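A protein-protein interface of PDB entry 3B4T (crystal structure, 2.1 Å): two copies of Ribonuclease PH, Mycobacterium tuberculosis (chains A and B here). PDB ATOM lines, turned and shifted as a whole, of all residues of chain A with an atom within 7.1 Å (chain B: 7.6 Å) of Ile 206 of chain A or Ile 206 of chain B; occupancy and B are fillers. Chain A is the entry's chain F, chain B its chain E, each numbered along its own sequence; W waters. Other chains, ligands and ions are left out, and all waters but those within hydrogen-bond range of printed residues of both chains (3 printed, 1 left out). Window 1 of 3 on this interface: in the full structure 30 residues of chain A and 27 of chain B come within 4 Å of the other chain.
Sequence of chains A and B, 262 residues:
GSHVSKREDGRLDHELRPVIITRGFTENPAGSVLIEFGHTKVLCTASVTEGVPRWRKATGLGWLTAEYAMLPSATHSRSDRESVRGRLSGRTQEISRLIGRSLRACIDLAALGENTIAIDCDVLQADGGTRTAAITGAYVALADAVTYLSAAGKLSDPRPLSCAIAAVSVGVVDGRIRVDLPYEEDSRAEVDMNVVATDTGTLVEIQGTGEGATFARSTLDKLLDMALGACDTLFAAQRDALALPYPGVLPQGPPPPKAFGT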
ATOM      1  N   LEU A  98     -14.147 -34.768  -7.280  1.00  0.00           N
ATOM      2  CA  LEU A  98     -14.707 -33.761  -6.378  1.00  0.00           C
ATOM      3  C   LEU A  98     -13.957 -33.715  -5.048  1.00  0.00           C
ATOM      4  O   LEU A  98     -13.534 -32.650  -4.601  1.00  0.00           O
ATOM      5  CB  LEU A  98     -16.192 -34.028  -6.127  1.00  0.00           C
ATOM      6  CG  LEU A  98     -16.845 -33.222  -4.999  1.00  0.00           C
ATOM      7  CD1 LEU A  98     -16.875 -31.744  -5.347  1.00  0.00           C
ATOM      8  CD2 LEU A  98     -18.250 -33.737  -4.720  1.00  0.00           C
ATOM      9  N   ARG A 101     -10.372 -32.258  -5.455  1.00  0.00           N
ATOM     10  CA  ARG A 101     -10.436 -30.804  -5.579  1.00  0.00           C
ATOM     11  C   ARG A 101     -10.724 -30.157  -4.226  1.00  0.00           C
ATOM     12  O   ARG A 101     -10.012 -29.250  -3.796  1.00  0.00           O
ATOM     13  CB  ARG A 101     -11.513 -30.386  -6.587  1.00  0.00           C
ATOM     14  CG  ARG A 101     -11.201 -30.738  -8.033  1.00  0.00           C
ATOM     15  CD  ARG A 101     -12.119 -30.000  -8.999  1.00  0.00           C
ATOM     16  NE  ARG A 101     -13.525 -30.361  -8.834  1.00  0.00           N
ATOM     17  CZ  ARG A 101     -14.153 -31.286  -9.556  1.00  0.00           C
ATOM     18  NH1 ARG A 101     -13.503 -31.953 -10.502  1.00  0.00           N
ATOM     19  NH2 ARG A 101     -15.434 -31.545  -9.334  1.00  0.00           N
ATOM     20  N   VAL A 170     -28.004 -30.084  -0.095  1.00  0.00           N
ATOM     21  CA  VAL A 170     -29.181 -29.245   0.088  1.00  0.00           C
ATOM     22  C   VAL A 170     -30.087 -29.369  -1.125  1.00  0.00           C
ATOM     23  O   VAL A 170     -29.630 -29.680  -2.223  1.00  0.00           O
ATOM     24  CB  VAL A 170     -28.809 -27.763   0.281  1.00  0.00           C
ATOM     25  CG1 VAL A 170     -28.228 -27.532   1.665  1.00  0.00           C
ATOM     26  CG2 VAL A 170     -27.839 -27.308  -0.801  1.00  0.00           C
ATOM     27  N   ASP A 192     -31.549 -30.844  -6.455  1.00  0.00           N
ATOM     28  CA  ASP A 192     -30.526 -31.360  -5.554  1.00  0.00           C
ATOM     29  C   ASP A 192     -29.182 -30.716  -5.828  1.00  0.00           C
ATOM     30  O   ASP A 192     -28.940 -30.214  -6.923  1.00  0.00           O
ATOM     31  CB  ASP A 192     -30.380 -32.872  -5.735  1.00  0.00           C
ATOM     32  CG  ASP A 192     -31.373 -33.655  -4.913  1.00  0.00           C
ATOM     33  OD1 ASP A 192     -32.068 -34.519  -5.487  1.00  0.00           O
ATOM     34  OD2 ASP A 192     -31.461 -33.403  -3.693  1.00  0.00           O
ATOM     35  N   MET A 193     -28.308 -30.737  -4.829  1.00  0.00           N
ATOM     36  CA  MET A 193     -26.909 -30.388  -5.044  1.00  0.00           C
ATOM     37  C   MET A 193     -26.063 -30.492  -3.783  1.00  0.00           C
ATOM     38  O   MET A 193     -26.580 -30.647  -2.675  1.00  0.00           O
ATOM     39  CB  MET A 193     -26.770 -29.001  -5.671  1.00  0.00           C
ATOM     40  CG  MET A 193     -27.229 -27.861  -4.792  1.00  0.00           C
ATOM     41  SD  MET A 193     -27.446 -26.374  -5.786  1.00  0.00           S
ATOM     42  CE  MET A 193     -28.864 -26.837  -6.775  1.00  0.00           C
ATOM     43  N   ASN A 194     -24.753 -30.402  -3.975  1.00  0.00           N
ATOM     44  CA  ASN A 194     -23.790 -30.556  -2.898  1.00  0.00           C
ATOM     45  C   ASN A 194     -22.898 -29.328  -2.793  1.00  0.00           C
ATOM     46  O   ASN A 194     -22.338 -28.871  -3.789  1.00  0.00           O
ATOM     47  CB  ASN A 194     -22.943 -31.805  -3.141  1.00  0.00           C
ATOM     48  CG  ASN A 194     -23.789 -33.043  -3.352  1.00  0.00           C
ATOM     49  OD1 ASN A 194     -24.518 -33.470  -2.459  1.00  0.00           O
ATOM     50  ND2 ASN A 194     -23.699 -33.624  -4.541  1.00  0.00           N
ATOM     51  N   VAL A 195     -22.771 -28.796  -1.583  1.00  0.00           N
ATOM     52  CA  VAL A 195     -21.985 -27.591  -1.360  1.00  0.00           C
ATOM     53  C   VAL A 195     -20.766 -27.880  -0.497  1.00  0.00           C
ATOM     54  O   VAL A 195     -20.874 -28.499   0.562  1.00  0.00           O
ATOM     55  CB  VAL A 195     -22.828 -26.488  -0.687  1.00  0.00           C
ATOM     56  CG1 VAL A 195     -21.957 -25.296  -0.324  1.00  0.00           C
ATOM     57  CG2 VAL A 195     -23.972 -26.068  -1.594  1.00  0.00           C
ATOM     58  N   VAL A 196     -19.606 -27.430  -0.956  1.00  0.00           N
ATOM     59  CA  VAL A 196     -18.374 -27.576  -0.200  1.00  0.00           C
ATOM     60  C   VAL A 196     -17.868 -26.195   0.175  1.00  0.00           C
ATOM     61  O   VAL A 196     -17.801 -25.300  -0.672  1.00  0.00           O
ATOM     62  CB  VAL A 196     -17.289 -28.304  -1.016  1.00  0.00           C
ATOM     63  CG1 VAL A 196     -16.109 -28.663  -0.124  1.00  0.00           C
ATOM     64  CG2 VAL A 196     -17.864 -29.553  -1.676  1.00  0.00           C
ATOM     65  N   LEU A 203     -16.154 -20.307  -0.299  1.00  0.00           N
ATOM     66  CA  LEU A 203     -16.752 -21.466  -0.949  1.00  0.00           C
ATOM     67  C   LEU A 203     -15.690 -22.282  -1.671  1.00  0.00           C
ATOM     68  O   LEU A 203     -14.612 -21.776  -1.978  1.00  0.00           O
ATOM     69  CB  LEU A 203     -17.831 -21.031  -1.944  1.00  0.00           C
ATOM     70  CG  LEU A 203     -19.100 -20.410  -1.355  1.00  0.00           C
ATOM     71  CD1 LEU A 203     -19.988 -19.840  -2.452  1.00  0.00           C
ATOM     72  CD2 LEU A 203     -19.856 -21.433  -0.520  1.00  0.00           C
ATOM     73  N   VAL A 204     -16.001 -23.545  -1.945  1.00  0.00           N
ATOM     74  CA  VAL A 204     -15.068 -24.421  -2.647  1.00  0.00           C
ATOM     75  C   VAL A 204     -15.674 -24.968  -3.931  1.00  0.00           C
ATOM     76  O   VAL A 204     -15.043 -24.933  -4.988  1.00  0.00           O
ATOM     77  CB  VAL A 204     -14.618 -25.599  -1.767  1.00  0.00           C
ATOM     78  CG1 VAL A 204     -13.581 -26.437  -2.502  1.00  0.00           C
ATOM     79  CG2 VAL A 204     -14.058 -25.089  -0.450  1.00  0.00           C
ATOM     80  N   GLU A 205     -16.900 -25.474  -3.842  1.00  0.00           N
ATOM     81  CA  GLU A 205     -17.569 -26.004  -5.019  1.00  0.00           C
ATOM     82  C   GLU A 205     -19.056 -26.261  -4.795  1.00  0.00           C
ATOM     83  O   GLU A 205     -19.487 -26.584  -3.687  1.00  0.00           O
ATOM     84  CB  GLU A 205     -16.878 -27.288  -5.494  1.00  0.00           C
ATOM     85  CG  GLU A 205     -17.515 -27.918  -6.722  1.00  0.00           C
ATOM     86  CD  GLU A 205     -16.612 -28.926  -7.404  1.00  0.00           C
ATOM     87  OE1 GLU A 205     -17.131 -29.746  -8.191  1.00  0.00           O
ATOM     88  OE2 GLU A 205     -15.386 -28.898  -7.155  1.00  0.00           O
ATOM     89  N   ILE A 206     -19.830 -26.096  -5.863  1.00  0.00           N
ATOM     90  CA  ILE A 206     -21.234 -26.474  -5.887  1.00  0.00           C
ATOM     91  C   ILE A 206     -21.365 -27.511  -6.989  1.00  0.00           C
ATOM     92  O   ILE A 206     -20.894 -27.290  -8.104  1.00  0.00           O
ATOM     93  CB  ILE A 206     -22.132 -25.264  -6.202  1.00  0.00           C
ATOM     94  CG1 ILE A 206     -21.800 -24.098  -5.266  1.00  0.00           C
ATOM     95  CG2 ILE A 206     -23.604 -25.646  -6.105  1.00  0.00           C
ATOM     96  CD1 ILE A 206     -22.445 -22.788  -5.671  1.00  0.00           C
ATOM     97  N   GLN A 207     -21.991 -28.643  -6.688  1.00  0.00           N
ATOM     98  CA  GLN A 207     -21.866 -29.801  -7.566  1.00  0.00           C
ATOM     99  C   GLN A 207     -23.084 -30.721  -7.581  1.00  0.00           C
ATOM    100  O   GLN A 207     -23.814 -30.833  -6.595  1.00  0.00           O
ATOM    101  CB  GLN A 207     -20.618 -30.602  -7.170  1.00  0.00           C
ATOM    102  CG  GLN A 207     -20.190 -31.668  -8.165  1.00  0.00           C
ATOM    103  CD  GLN A 207     -20.985 -32.952  -8.035  1.00  0.00           C
ATOM    104  OE1 GLN A 207     -21.558 -33.239  -6.986  1.00  0.00           O
ATOM    105  NE2 GLN A 207     -21.021 -33.734  -9.107  1.00  0.00           N
ATOM    106  N   GLY A 208     -23.291 -31.374  -8.720  1.00  0.00           N
ATOM    107  CA  GLY A 208     -24.247 -32.462  -8.829  1.00  0.00           C
ATOM    108  C   GLY A 208     -25.699 -32.094  -8.607  1.00  0.00           C
ATOM    109  O   GLY A 208     -26.300 -32.482  -7.605  1.00  0.00           O
ATOM    110  N   THR A 209     -26.270 -31.354  -9.552  1.00  0.00           N
ATOM    111  CA  THR A 209     -27.691 -31.036  -9.507  1.00  0.00           C
ATOM    112  C   THR A 209     -28.503 -32.295  -9.795  1.00  0.00           C
ATOM    113  O   THR A 209     -28.114 -33.116 -10.628  1.00  0.00           O
ATOM    114  CB  THR A 209     -28.058 -29.924 -10.511  1.00  0.00           C
ATOM    115  OG1 THR A 209     -27.219 -28.783 -10.289  1.00  0.00           O
ATOM    116  CG2 THR A 209     -29.518 -29.518 -10.349  1.00  0.00           C
ATOM    117  N   PHE A 215     -32.826 -24.691 -11.510  1.00  0.00           N
ATOM    118  CA  PHE A 215     -33.111 -23.802 -10.392  1.00  0.00           C
ATOM    119  C   PHE A 215     -32.820 -22.334 -10.691  1.00  0.00           C
ATOM    120  O   PHE A 215     -31.840 -22.003 -11.357  1.00  0.00           O
ATOM    121  CB  PHE A 215     -32.340 -24.249  -9.147  1.00  0.00           C
ATOM    122  CG  PHE A 215     -30.863 -24.417  -9.373  1.00  0.00           C
ATOM    123  CD1 PHE A 215     -30.366 -25.558  -9.980  1.00  0.00           C
ATOM    124  CD2 PHE A 215     -29.970 -23.440  -8.967  1.00  0.00           C
ATOM    125  CE1 PHE A 215     -29.009 -25.717 -10.185  1.00  0.00           C
ATOM    126  CE2 PHE A 215     -28.611 -23.594  -9.169  1.00  0.00           C
ATOM    127  CZ  PHE A 215     -28.131 -24.734  -9.779  1.00  0.00           C
ATOM    128  N   LEU A 220     -30.887 -20.654  -5.718  1.00  0.00           N
ATOM    129  CA  LEU A 220     -29.487 -20.940  -5.436  1.00  0.00           C
ATOM    130  C   LEU A 220     -29.027 -20.236  -4.164  1.00  0.00           C
ATOM    131  O   LEU A 220     -28.348 -20.829  -3.328  1.00  0.00           O
ATOM    132  CB  LEU A 220     -28.605 -20.520  -6.612  1.00  0.00           C
ATOM    133  CG  LEU A 220     -27.096 -20.654  -6.391  1.00  0.00           C
ATOM    134  CD1 LEU A 220     -26.752 -22.042  -5.874  1.00  0.00           C
ATOM    135  CD2 LEU A 220     -26.330 -20.349  -7.674  1.00  0.00           C
ATOM    136  N   LEU A 224     -27.738 -21.944  -0.819  1.00  0.00           N
ATOM    137  CA  LEU A 224     -26.415 -21.608  -0.310  1.00  0.00           C
ATOM    138  C   LEU A 224     -26.483 -21.150   1.144  1.00  0.00           C
ATOM    139  O   LEU A 224     -25.684 -21.585   1.971  1.00  0.00           O
ATOM    140  CB  LEU A 224     -25.749 -20.537  -1.175  1.00  0.00           C
ATOM    141  CG  LEU A 224     -25.293 -20.970  -2.570  1.00  0.00           C
ATOM    142  CD1 LEU A 224     -24.522 -19.847  -3.246  1.00  0.00           C
ATOM    143  CD2 LEU A 224     -24.450 -22.239  -2.500  1.00  0.00           C
ATOM    144  N   LEU B  98     -22.287 -34.827 -17.239  1.00  0.00           N
ATOM    145  CA  LEU B  98     -22.797 -33.459 -17.223  1.00  0.00           C
ATOM    146  C   LEU B  98     -23.579 -33.126 -18.494  1.00  0.00           C
ATOM    147  O   LEU B  98     -24.652 -32.525 -18.430  1.00  0.00           O
ATOM    148  CB  LEU B  98     -21.656 -32.460 -17.038  1.00  0.00           C
ATOM    149  CG  LEU B  98     -22.039 -30.983 -17.185  1.00  0.00           C
ATOM    150  CD1 LEU B  98     -23.005 -30.560 -16.088  1.00  0.00           C
ATOM    151  CD2 LEU B  98     -20.802 -30.096 -17.186  1.00  0.00           C
ATOM    152  N   ARG B 101     -27.016 -35.036 -18.487  1.00  0.00           N
ATOM    153  CA  ARG B 101     -27.973 -34.482 -17.539  1.00  0.00           C
ATOM    154  C   ARG B 101     -28.510 -33.137 -18.021  1.00  0.00           C
ATOM    155  O   ARG B 101     -29.719 -32.908 -18.029  1.00  0.00           O
ATOM    156  CB  ARG B 101     -27.343 -34.331 -16.153  1.00  0.00           C
ATOM    157  CG  ARG B 101     -28.278 -34.722 -15.023  1.00  0.00           C
ATOM    158  CD  ARG B 101     -27.783 -34.250 -13.666  1.00  0.00           C
ATOM    159  NE  ARG B 101     -26.327 -34.248 -13.558  1.00  0.00           N
ATOM    160  CZ  ARG B 101     -25.597 -33.146 -13.424  1.00  0.00           C
ATOM    161  NH1 ARG B 101     -26.189 -31.960 -13.378  1.00  0.00           N
ATOM    162  NH2 ARG B 101     -24.278 -33.226 -13.328  1.00  0.00           N
ATOM    163  N   VAL B 170     -16.288 -19.435 -17.216  1.00  0.00           N
ATOM    164  CA  VAL B 170     -16.023 -18.135 -16.615  1.00  0.00           C
ATOM    165  C   VAL B 170     -15.034 -18.319 -15.474  1.00  0.00           C
ATOM    166  O   VAL B 170     -14.984 -19.381 -14.860  1.00  0.00           O
ATOM    167  CB  VAL B 170     -17.315 -17.489 -16.076  1.00  0.00           C
ATOM    168  CG1 VAL B 170     -17.900 -18.331 -14.950  1.00  0.00           C
ATOM    169  CG2 VAL B 170     -17.048 -16.070 -15.605  1.00  0.00           C
ATOM    170  N   ASP B 192     -12.165 -20.817 -11.691  1.00  0.00           N
ATOM    171  CA  ASP B 192     -12.906 -20.912 -12.943  1.00  0.00           C
ATOM    172  C   ASP B 192     -13.915 -22.047 -12.903  1.00  0.00           C
ATOM    173  O   ASP B 192     -13.748 -23.015 -12.162  1.00  0.00           O
ATOM    174  CB  ASP B 192     -11.958 -21.079 -14.130  1.00  0.00           C
ATOM    175  CG  ASP B 192     -11.389 -22.474 -14.227  1.00  0.00           C
ATOM    176  OD1 ASP B 192     -10.223 -22.671 -13.831  1.00  0.00           O
ATOM    177  OD2 ASP B 192     -12.113 -23.376 -14.695  1.00  0.00           O
ATOM    178  N   MET B 193     -14.968 -21.916 -13.702  1.00  0.00           N
ATOM    179  CA  MET B 193     -16.030 -22.908 -13.710  1.00  0.00           C
ATOM    180  C   MET B 193     -16.827 -22.890 -15.003  1.00  0.00           C
ATOM    181  O   MET B 193     -16.671 -21.998 -15.841  1.00  0.00           O
ATOM    182  CB  MET B 193     -16.964 -22.687 -12.522  1.00  0.00           C
ATOM    183  CG  MET B 193     -17.674 -21.351 -12.546  1.00  0.00           C
ATOM    184  SD  MET B 193     -18.102 -20.806 -10.886  1.00  0.00           S
ATOM    185  CE  MET B 193     -16.480 -20.810 -10.123  1.00  0.00           C
ATOM    186  N   ASN B 194     -17.683 -23.892 -15.153  1.00  0.00           N
ATOM    187  CA  ASN B 194     -18.554 -23.995 -16.305  1.00  0.00           C
ATOM    188  C   ASN B 194     -20.001 -23.810 -15.881  1.00  0.00           C
ATOM    189  O   ASN B 194     -20.520 -24.561 -15.057  1.00  0.00           O
ATOM    190  CB  ASN B 194     -18.355 -25.344 -16.993  1.00  0.00           C
ATOM    191  CG  ASN B 194     -16.912 -25.581 -17.386  1.00  0.00           C
ATOM    192  OD1 ASN B 194     -16.326 -24.804 -18.137  1.00  0.00           O
ATOM    193  ND2 ASN B 194     -16.329 -26.656 -16.873  1.00  0.00           N
ATOM    194  N   VAL B 195     -20.642 -22.792 -16.441  1.00  0.00           N
ATOM    195  CA  VAL B 195     -22.023 -22.487 -16.114  1.00  0.00           C
ATOM    196  C   VAL B 195     -22.950 -23.031 -17.188  1.00  0.00           C
ATOM    197  O   VAL B 195     -22.819 -22.695 -18.365  1.00  0.00           O
ATOM    198  CB  VAL B 195     -22.238 -20.972 -15.973  1.00  0.00           C
ATOM    199  CG1 VAL B 195     -23.698 -20.668 -15.690  1.00  0.00           C
ATOM    200  CG2 VAL B 195     -21.348 -20.419 -14.873  1.00  0.00           C
ATOM    201  N   VAL B 196     -23.877 -23.886 -16.779  1.00  0.00           N
ATOM    202  CA  VAL B 196     -24.859 -24.435 -17.700  1.00  0.00           C
ATOM    203  C   VAL B 196     -26.220 -23.822 -17.401  1.00  0.00           C
ATOM    204  O   VAL B 196     -26.763 -23.991 -16.310  1.00  0.00           O
ATOM    205  CB  VAL B 196     -24.934 -25.968 -17.602  1.00  0.00           C
ATOM    206  CG1 VAL B 196     -25.943 -26.516 -18.600  1.00  0.00           C
ATOM    207  CG2 VAL B 196     -23.561 -26.576 -17.840  1.00  0.00           C
ATOM    208  N   LEU B 203     -30.783 -22.208 -13.929  1.00  0.00           N
ATOM    209  CA  LEU B 203     -29.457 -22.804 -13.988  1.00  0.00           C
ATOM    210  C   LEU B 203     -29.562 -24.321 -13.925  1.00  0.00           C
ATOM    211  O   LEU B 203     -30.446 -24.861 -13.259  1.00  0.00           O
ATOM    212  CB  LEU B 203     -28.602 -22.302 -12.825  1.00  0.00           C
ATOM    213  CG  LEU B 203     -28.223 -20.821 -12.820  1.00  0.00           C
ATOM    214  CD1 LEU B 203     -28.024 -20.324 -11.399  1.00  0.00           C
ATOM    215  CD2 LEU B 203     -26.974 -20.590 -13.657  1.00  0.00           C
ATOM    216  N   VAL B 204     -28.657 -25.007 -14.614  1.00  0.00           N
ATOM    217  CA  VAL B 204     -28.624 -26.464 -14.583  1.00  0.00           C
ATOM    218  C   VAL B 204     -27.472 -26.974 -13.730  1.00  0.00           C
ATOM    219  O   VAL B 204     -27.613 -27.959 -13.003  1.00  0.00           O
ATOM    220  CB  VAL B 204     -28.507 -27.062 -15.995  1.00  0.00           C
ATOM    221  CG1 VAL B 204     -28.209 -28.554 -15.914  1.00  0.00           C
ATOM    222  CG2 VAL B 204     -29.781 -26.810 -16.782  1.00  0.00           C
ATOM    223  N   GLU B 205     -26.334 -26.295 -13.809  1.00  0.00           N
ATOM    224  CA  GLU B 205     -25.138 -26.742 -13.109  1.00  0.00           C
ATOM    225  C   GLU B 205     -24.071 -25.658 -13.100  1.00  0.00           C
ATOM    226  O   GLU B 205     -23.973 -24.865 -14.037  1.00  0.00           O
ATOM    227  CB  GLU B 205     -24.578 -28.003 -13.779  1.00  0.00           C
ATOM    228  CG  GLU B 205     -23.295 -28.545 -13.151  1.00  0.00           C
ATOM    229  CD  GLU B 205     -23.553 -29.671 -12.164  1.00  0.00           C
ATOM    230  OE1 GLU B 205     -24.648 -30.267 -12.217  1.00  0.00           O
ATOM    231  OE2 GLU B 205     -22.660 -29.964 -11.339  1.00  0.00           O
ATOM    232  N   ILE B 206     -23.279 -25.632 -12.033  1.00  0.00           N
ATOM    233  CA  ILE B 206     -22.090 -24.793 -11.955  1.00  0.00           C
ATOM    234  C   ILE B 206     -20.885 -25.679 -11.644  1.00  0.00           C
ATOM    235  O   ILE B 206     -20.563 -25.912 -10.481  1.00  0.00           O
ATOM    236  CB  ILE B 206     -22.221 -23.730 -10.854  1.00  0.00           C
ATOM    237  CG1 ILE B 206     -23.488 -22.897 -11.056  1.00  0.00           C
ATOM    238  CG2 ILE B 206     -20.993 -22.836 -10.830  1.00  0.00           C
ATOM    239  CD1 ILE B 206     -23.824 -22.027  -9.870  1.00  0.00           C
ATOM    240  N   GLN B 207     -20.220 -26.167 -12.686  1.00  0.00           N
ATOM    241  CA  GLN B 207     -19.186 -27.189 -12.523  1.00  0.00           C
ATOM    242  C   GLN B 207     -17.803 -26.631 -12.185  1.00  0.00           C
ATOM    243  O   GLN B 207     -17.213 -25.892 -12.976  1.00  0.00           O
ATOM    244  CB  GLN B 207     -19.092 -28.050 -13.783  1.00  0.00           C
ATOM    245  CG  GLN B 207     -18.176 -29.249 -13.636  1.00  0.00           C
ATOM    246  CD  GLN B 207     -17.803 -29.867 -14.967  1.00  0.00           C
ATOM    247  OE1 GLN B 207     -17.587 -29.163 -15.952  1.00  0.00           O
ATOM    248  NE2 GLN B 207     -17.721 -31.191 -15.001  1.00  0.00           N
ATOM    249  N   GLY B 208     -17.290 -26.994 -11.012  1.00  0.00           N
ATOM    250  CA  GLY B 208     -15.924 -26.665 -10.643  1.00  0.00           C
ATOM    251  C   GLY B 208     -14.977 -27.501 -11.480  1.00  0.00           C
ATOM    252  O   GLY B 208     -15.343 -28.589 -11.926  1.00  0.00           O
ATOM    253  N   THR B 209     -13.759 -27.010 -11.699  1.00  0.00           N
ATOM    254  CA  THR B 209     -12.866 -27.655 -12.662  1.00  0.00           C
ATOM    255  C   THR B 209     -11.392 -27.726 -12.257  1.00  0.00           C
ATOM    256  O   THR B 209     -10.713 -28.710 -12.551  1.00  0.00           O
ATOM    257  CB  THR B 209     -12.945 -26.952 -14.024  1.00  0.00           C
ATOM    258  OG1 THR B 209     -12.425 -25.624 -13.899  1.00  0.00           O
ATOM    259  CG2 THR B 209     -14.386 -26.877 -14.503  1.00  0.00           C
ATOM    260  N   PHE B 215     -13.380 -19.420  -3.229  1.00  0.00           N
ATOM    261  CA  PHE B 215     -13.831 -18.110  -3.676  1.00  0.00           C
ATOM    262  C   PHE B 215     -14.934 -17.549  -2.782  1.00  0.00           C
ATOM    263  O   PHE B 215     -15.710 -18.299  -2.188  1.00  0.00           O
ATOM    264  CB  PHE B 215     -14.301 -18.173  -5.132  1.00  0.00           C
ATOM    265  CG  PHE B 215     -15.304 -19.260  -5.403  1.00  0.00           C
ATOM    266  CD1 PHE B 215     -14.890 -20.564  -5.626  1.00  0.00           C
ATOM    267  CD2 PHE B 215     -16.658 -18.976  -5.455  1.00  0.00           C
ATOM    268  CE1 PHE B 215     -15.810 -21.563  -5.881  1.00  0.00           C
ATOM    269  CE2 PHE B 215     -17.582 -19.972  -5.713  1.00  0.00           C
ATOM    270  CZ  PHE B 215     -17.157 -21.267  -5.925  1.00  0.00           C
ATOM    271  N   LEU B 220     -18.677 -15.294  -6.609  1.00  0.00           N
ATOM    272  CA  LEU B 220     -19.569 -16.226  -7.295  1.00  0.00           C
ATOM    273  C   LEU B 220     -20.665 -15.484  -8.049  1.00  0.00           C
ATOM    274  O   LEU B 220     -20.958 -15.796  -9.204  1.00  0.00           O
ATOM    275  CB  LEU B 220     -20.199 -17.214  -6.310  1.00  0.00           C
ATOM    276  CG  LEU B 220     -21.308 -18.097  -6.894  1.00  0.00           C
ATOM    277  CD1 LEU B 220     -20.780 -18.928  -8.057  1.00  0.00           C
ATOM    278  CD2 LEU B 220     -21.918 -18.994  -5.826  1.00  0.00           C
ATOM    279  N   LEU B 223     -19.268 -13.882 -11.172  1.00  0.00           N
ATOM    280  CA  LEU B 223     -19.019 -14.915 -12.170  1.00  0.00           C
ATOM    281  C   LEU B 223     -20.315 -15.343 -12.849  1.00  0.00           C
ATOM    282  O   LEU B 223     -20.367 -15.474 -14.072  1.00  0.00           O
ATOM    283  CB  LEU B 223     -18.331 -16.128 -11.535  1.00  0.00           C
ATOM    284  CG  LEU B 223     -16.906 -15.919 -11.021  1.00  0.00           C
ATOM    285  CD1 LEU B 223     -16.451 -17.114 -10.197  1.00  0.00           C
ATOM    286  CD2 LEU B 223     -15.950 -15.658 -12.179  1.00  0.00           C
ATOM    287  N   LEU B 224     -21.355 -15.558 -12.049  1.00  0.00           N
ATOM    288  CA  LEU B 224     -22.660 -15.946 -12.576  1.00  0.00           C
ATOM    289  C   LEU B 224     -23.284 -14.843 -13.430  1.00  0.00           C
ATOM    290  O   LEU B 224     -23.864 -15.117 -14.480  1.00  0.00           O
ATOM    291  CB  LEU B 224     -23.610 -16.337 -11.442  1.00  0.00           C
ATOM    292  CG  LEU B 224     -23.249 -17.608 -10.669  1.00  0.00           C
ATOM    293  CD1 LEU B 224     -24.233 -17.846  -9.531  1.00  0.00           C
ATOM    294  CD2 LEU B 224     -23.203 -18.811 -11.603  1.00  0.00           C
HETATM  295  O   HOH W   1     -23.088 -27.273  -9.742  1.00  0.00           O
HETATM  296  O   HOH W   2     -26.916 -35.823 -10.816  1.00  0.00           O
HETATM  297  O   HOH W   3     -16.988 -31.677 -12.155  1.00  0.00           O
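Leu 203 of chain A touches Phe 215 of chain B, and with the chains exchanged Phe 215 of chain A touches Leu 203 of chain B.
Val 204 of chain A touches Phe 215 of chain B, and with the chains exchanged Phe 215 of chain A touches Val 204 of chain B.
Glu 205 of chain A touches Gly 208 of chain B, and with the chains exchanged Gly 208 of chain A touches Glu 205 of chain B.
N of Leu 203 of chain B is in hydrogen-bond range of O of Phe 215 of chain A (2.8 Å).
O of Val 204 of chain B lies within hydrogen-bond range of OG1 of Thr 209 of chain A, at 2.9 Å.
The backbone NH (N) of Gly 208 of chain A sits at hydrogen-bond distance from the side-chain carboxylate (OE2) of Glu 205 of chain B (3.0 Å).
The side-chain carboxylate of Glu 205 of chain B is in hydrogen-bond range of the backbone NH of Thr 209 of chain A (3.3 Å).
O of Phe 215 of chain B is in hydrogen-bond range of N of Leu 203 of chain A (2.8 Å).
The backbone carbonyl oxygen (O) of Ile 206 of chain A sits close to the backbone carbonyl oxygen (O) of Ile 206 of chain B.
Leu 203 of chain A touches Leu 220 of chain B.
Val 204 of chain A touches Phe 215 of chain B (O to CE1, 3.6 Å).
Glu 205 of chain A touches Gly 208 of chain B.
Leu 220 of chain B touches Ile 206 of chain A (CD2 to CD1, 3.8 Å).
Gln 207 of chain A touches Glu 205 of chain B (C to OE2, 3.9 Å).
CD of Arg 101 of chain B touches O of Thr 209 of chain A (3.3 Å).
CD2 of Leu 220 of chain A touches CD1 of Leu 224 of chain B (3.8 Å).
CD2 of Leu 220 of chain B touches CD1 of Leu 224 of chain A, at 3.8 Å.
Of chain B, only Ile 206 (2.8 Å) and Leu 220 (3.8 Å) come within 4 Å of Ile 206 of chain A.
Printed residues of chain A within 4 Å of Ile 206 of chain B: Ile 206 (2.8 Å) and Leu 220 (3.7 Å).
Printed residues of chain B within 4 Å of Leu 224 of chain A: Leu 220.
Printed residues of chain A within 4 Å of Phe 215 of chain B: Leu 203 (2.8 Å) and Val 204 (3.6 Å).
The nearest residue of chain B that does not touch Ile 206 of chain A is Glu 205 of chain B (4.6 Å).
The nearest residue of chain A that does not touch Ile 206 of chain B is Gln 207 of chain A (4.9 Å).
Hydrophobic or aromatic side chains of chain A within 4 Å of the printed part of chain B: Leu 203, Ile 206, Phe 215, Leu 220 and Leu 224.
Of the 19 printed residues of chain B, 9 touch a printed residue of chain A.
Among the printed residues, 17 pairs touch across the chains.
Among the printed residues, no Asp or Glu carboxylate lies within 4 Å of a Lys or Arg side-chain nitrogen of the other chain.
NH1 of Arg 101 of chain B is in salt-bridge range of OE1 of Glu 205 of chain B, at 2.6 Å.
The backbone NH of Val 196 of chain B is in hydrogen-bond range of the backbone carbonyl oxygen of Glu 205 of chain B, at 2.9 Å.
N of Asn 194 of chain A is in hydrogen-bond range of O of Gln 207 of chain A (2.8 Å).
N of Val 204 of chain A lies within hydrogen-bond range of O of Val 196 of chain A (2.8 Å).
Water W1 lies within hydrogen-bond range of the backbone carbonyl oxygen (O) of Ile 206 of chain A (2.7 Å), the backbone NH (N) of Ile 206 of chain B (2.8 Å) and the side-chain carboxylate (OE2) of Glu 205 of chain B (3.2 Å).
Water W2 bridges O of Thr 209 of chain A and NE of Arg 101 of chain B.
Water W3 bridges NE2 of Gln 207 of chain B (3.0 Å) and NH2 of Arg 101 of chain A (3.2 Å).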
